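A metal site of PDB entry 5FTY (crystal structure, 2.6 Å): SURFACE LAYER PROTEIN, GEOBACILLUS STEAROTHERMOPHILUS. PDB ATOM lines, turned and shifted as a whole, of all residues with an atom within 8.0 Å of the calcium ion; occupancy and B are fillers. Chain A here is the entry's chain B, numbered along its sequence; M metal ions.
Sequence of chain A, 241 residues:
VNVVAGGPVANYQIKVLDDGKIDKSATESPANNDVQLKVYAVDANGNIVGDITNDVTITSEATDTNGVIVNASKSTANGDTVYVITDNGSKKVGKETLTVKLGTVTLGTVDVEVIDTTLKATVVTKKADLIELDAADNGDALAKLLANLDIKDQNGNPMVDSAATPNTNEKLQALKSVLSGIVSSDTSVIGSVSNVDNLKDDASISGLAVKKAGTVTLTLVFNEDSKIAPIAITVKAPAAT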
ATOM      1  N   VAL A 160     -10.958  15.014   6.932  1.00  0.00           N
ATOM      2  CA  VAL A 160      -9.988  13.956   7.206  1.00  0.00           C
ATOM      3  C   VAL A 160     -10.648  12.606   7.474  1.00  0.00           C
ATOM      4  O   VAL A 160     -11.737  12.539   8.054  1.00  0.00           O
ATOM      5  CB  VAL A 160      -9.083  14.371   8.400  1.00  0.00           C
ATOM      6  CG1 VAL A 160      -8.809  13.202   9.345  1.00  0.00           C
ATOM      7  CG2 VAL A 160      -7.778  14.989   7.896  1.00  0.00           C
ATOM      8  N   ASP A 161      -9.994  11.528   7.020  1.00  0.00           N
ATOM      9  CA  ASP A 161     -10.448  10.178   7.310  1.00  0.00           C
ATOM     10  C   ASP A 161     -10.513   9.916   8.814  1.00  0.00           C
ATOM     11  O   ASP A 161      -9.505   9.998   9.508  1.00  0.00           O
ATOM     12  CB  ASP A 161      -9.525   9.147   6.651  1.00  0.00           C
ATOM     13  CG  ASP A 161      -9.927   7.717   6.956  1.00  0.00           C
ATOM     14  OD1 ASP A 161     -11.143   7.453   7.035  1.00  0.00           O
ATOM     15  OD2 ASP A 161      -9.029   6.855   7.111  1.00  0.00           O
ATOM     16  N   SER A 162     -11.711   9.597   9.298  1.00  0.00           N
ATOM     17  CA  SER A 162     -11.913   9.306  10.706  1.00  0.00           C
ATOM     18  C   SER A 162     -11.923   7.806  10.941  1.00  0.00           C
ATOM     19  O   SER A 162     -12.651   7.064  10.275  1.00  0.00           O
ATOM     20  CB  SER A 162     -13.218   9.922  11.199  1.00  0.00           C
ATOM     21  OG  SER A 162     -13.336   9.806  12.609  1.00  0.00           O
ATOM     22  N   ALA A 163     -11.114   7.345  11.893  1.00  0.00           N
ATOM     23  CA  ALA A 163     -10.969   5.922  12.168  1.00  0.00           C
ATOM     24  C   ALA A 163     -12.193   5.317  12.854  1.00  0.00           C
ATOM     25  O   ALA A 163     -12.263   4.109  13.057  1.00  0.00           O
ATOM     26  CB  ALA A 163      -9.710   5.657  12.983  1.00  0.00           C
ATOM     27  N   ALA A 164     -13.142   6.171  13.214  1.00  0.00           N
ATOM     28  CA  ALA A 164     -14.417   5.702  13.771  1.00  0.00           C
ATOM     29  C   ALA A 164     -15.156   4.882  12.719  1.00  0.00           C
ATOM     30  O   ALA A 164     -15.959   4.013  13.059  1.00  0.00           O
ATOM     31  CB  ALA A 164     -15.264   6.875  14.234  1.00  0.00           C
ATOM     32  N   THR A 165     -14.887   5.162  11.448  1.00  0.00           N
ATOM     33  CA  THR A 165     -15.530   4.448  10.360  1.00  0.00           C
ATOM     34  C   THR A 165     -14.480   3.735   9.506  1.00  0.00           C
ATOM     35  O   THR A 165     -13.990   4.293   8.540  1.00  0.00           O
ATOM     36  CB  THR A 165     -16.341   5.407   9.465  1.00  0.00           C
ATOM     37  OG1 THR A 165     -15.456   6.387   8.889  1.00  0.00           O
ATOM     38  CG2 THR A 165     -17.416   6.116  10.265  1.00  0.00           C
ATOM     39  N   PRO A 166     -14.148   2.491   9.882  1.00  0.00           N
ATOM     40  CA  PRO A 166     -13.075   1.732   9.208  1.00  0.00           C
ATOM     41  C   PRO A 166     -13.333   1.520   7.724  1.00  0.00           C
ATOM     42  O   PRO A 166     -12.376   1.414   6.953  1.00  0.00           O
ATOM     43  CB  PRO A 166     -13.110   0.388   9.949  1.00  0.00           C
ATOM     44  CG  PRO A 166     -13.705   0.695  11.265  1.00  0.00           C
ATOM     45  CD  PRO A 166     -14.735   1.746  11.003  1.00  0.00           C
ATOM     46  N   ASN A 167     -14.599   1.463   7.326  1.00  0.00           N
ATOM     47  CA  ASN A 167     -14.939   1.059   5.967  1.00  0.00           C
ATOM     48  C   ASN A 167     -15.164   2.217   4.979  1.00  0.00           C
ATOM     49  O   ASN A 167     -15.473   1.983   3.821  1.00  0.00           O
ATOM     50  CB  ASN A 167     -16.169   0.148   5.984  1.00  0.00           C
ATOM     51  CG  ASN A 167     -15.993  -1.049   6.912  1.00  0.00           C
ATOM     52  OD1 ASN A 167     -16.820  -1.299   7.784  1.00  0.00           O
ATOM     53  ND2 ASN A 167     -14.913  -1.800   6.722  1.00  0.00           N
ATOM     54  N   THR A 168     -14.995   3.452   5.447  1.00  0.00           N
ATOM     55  CA  THR A 168     -15.156   4.603   4.565  1.00  0.00           C
ATOM     56  C   THR A 168     -14.211   5.775   4.871  1.00  0.00           C
ATOM     57  O   THR A 168     -14.376   6.484   5.863  1.00  0.00           O
ATOM     58  CB  THR A 168     -16.625   5.091   4.500  1.00  0.00           C
ATOM     59  OG1 THR A 168     -16.692   6.348   3.810  1.00  0.00           O
ATOM     60  CG2 THR A 168     -17.209   5.250   5.896  1.00  0.00           C
ATOM     61  N   ASN A 169     -13.221   5.968   4.001  1.00  0.00           N
ATOM     62  CA  ASN A 169     -12.307   7.093   4.086  1.00  0.00           C
ATOM     63  C   ASN A 169     -13.034   8.386   3.751  1.00  0.00           C
ATOM     64  O   ASN A 169     -13.421   8.603   2.602  1.00  0.00           O
ATOM     65  CB  ASN A 169     -11.134   6.870   3.143  1.00  0.00           C
ATOM     66  CG  ASN A 169      -9.983   7.842   3.380  1.00  0.00           C
ATOM     67  OD1 ASN A 169     -10.182   9.059   3.441  1.00  0.00           O
ATOM     68  ND2 ASN A 169      -8.781   7.309   3.531  1.00  0.00           N
ATOM     69  N   GLU A 170     -13.224   9.249   4.748  1.00  0.00           N
ATOM     70  CA  GLU A 170     -13.939  10.506   4.548  1.00  0.00           C
ATOM     71  C   GLU A 170     -13.185  11.448   3.614  1.00  0.00           C
ATOM     72  O   GLU A 170     -13.790  12.153   2.810  1.00  0.00           O
ATOM     73  CB  GLU A 170     -14.195  11.211   5.881  1.00  0.00           C
ATOM     74  CG  GLU A 170     -15.276  10.581   6.736  1.00  0.00           C
ATOM     75  CD  GLU A 170     -14.802   9.347   7.476  1.00  0.00           C
ATOM     76  OE1 GLU A 170     -13.614   9.307   7.843  1.00  0.00           O
ATOM     77  OE2 GLU A 170     -15.624   8.431   7.698  1.00  0.00           O
ATOM     78  N   LYS A 171     -11.858  11.463   3.726  1.00  0.00           N
ATOM     79  CA  LYS A 171     -11.013  12.350   2.936  1.00  0.00           C
ATOM     80  C   LYS A 171     -11.110  12.042   1.443  1.00  0.00           C
ATOM     81  O   LYS A 171     -11.254  12.947   0.626  1.00  0.00           O
ATOM     82  CB  LYS A 171      -9.564  12.265   3.396  1.00  0.00           C
ATOM     83  CG  LYS A 171      -8.629  13.205   2.650  1.00  0.00           C
ATOM     84  CD  LYS A 171      -7.222  13.143   3.200  1.00  0.00           C
ATOM     85  CE  LYS A 171      -6.385  14.291   2.669  1.00  0.00           C
ATOM     86  NZ  LYS A 171      -4.988  14.274   3.197  1.00  0.00           N
ATOM     87  N   ASP A 201     -12.335   3.216  -2.040  1.00  0.00           N
ATOM     88  CA  ASP A 201     -12.336   3.269  -0.588  1.00  0.00           C
ATOM     89  C   ASP A 201     -12.453   1.848  -0.037  1.00  0.00           C
ATOM     90  O   ASP A 201     -13.405   1.538   0.669  1.00  0.00           O
ATOM     91  CB  ASP A 201     -13.510   4.116  -0.106  1.00  0.00           C
ATOM     92  CG  ASP A 201     -13.309   4.653   1.291  1.00  0.00           C
ATOM     93  OD1 ASP A 201     -12.486   4.083   2.053  1.00  0.00           O
ATOM     94  OD2 ASP A 201     -13.973   5.661   1.645  1.00  0.00           O
HETATM   95 CA    CA M   1     -12.991   6.298   7.874  1.00  0.00          CA
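N of Asn 169 touches the calcium ion, at 3.9 Å.
The nearest printed residue that does not touch the calcium ion is Pro 166 (4.5 Å).
OE1 of Glu 170 is in hydrogen-bond range of N of Ser 162 (2.4 Å).
The side-chain carboxylate of Asp 201 lies within hydrogen-bond range of the backbone NH of Asn 169 (2.5 Å).
N of Lys 171 sits at hydrogen-bond distance from OD1 of Asn 169 (2.9 Å).
OD1 of Asp 161 binds the calcium ion (2.3 Å).
The calcium ion is bound by O of Thr 165, 2.3 Å away.
The backbone carbonyl oxygen (O) of Thr 168 binds the calcium ion (2.4 Å).
The calcium ion is bound by O of Ser 162.
OG1 of Thr 165 binds the calcium ion (2.7 Å).
Slightly farther from the calcium ion lies OE1 of Glu 170 (3.1 Å).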
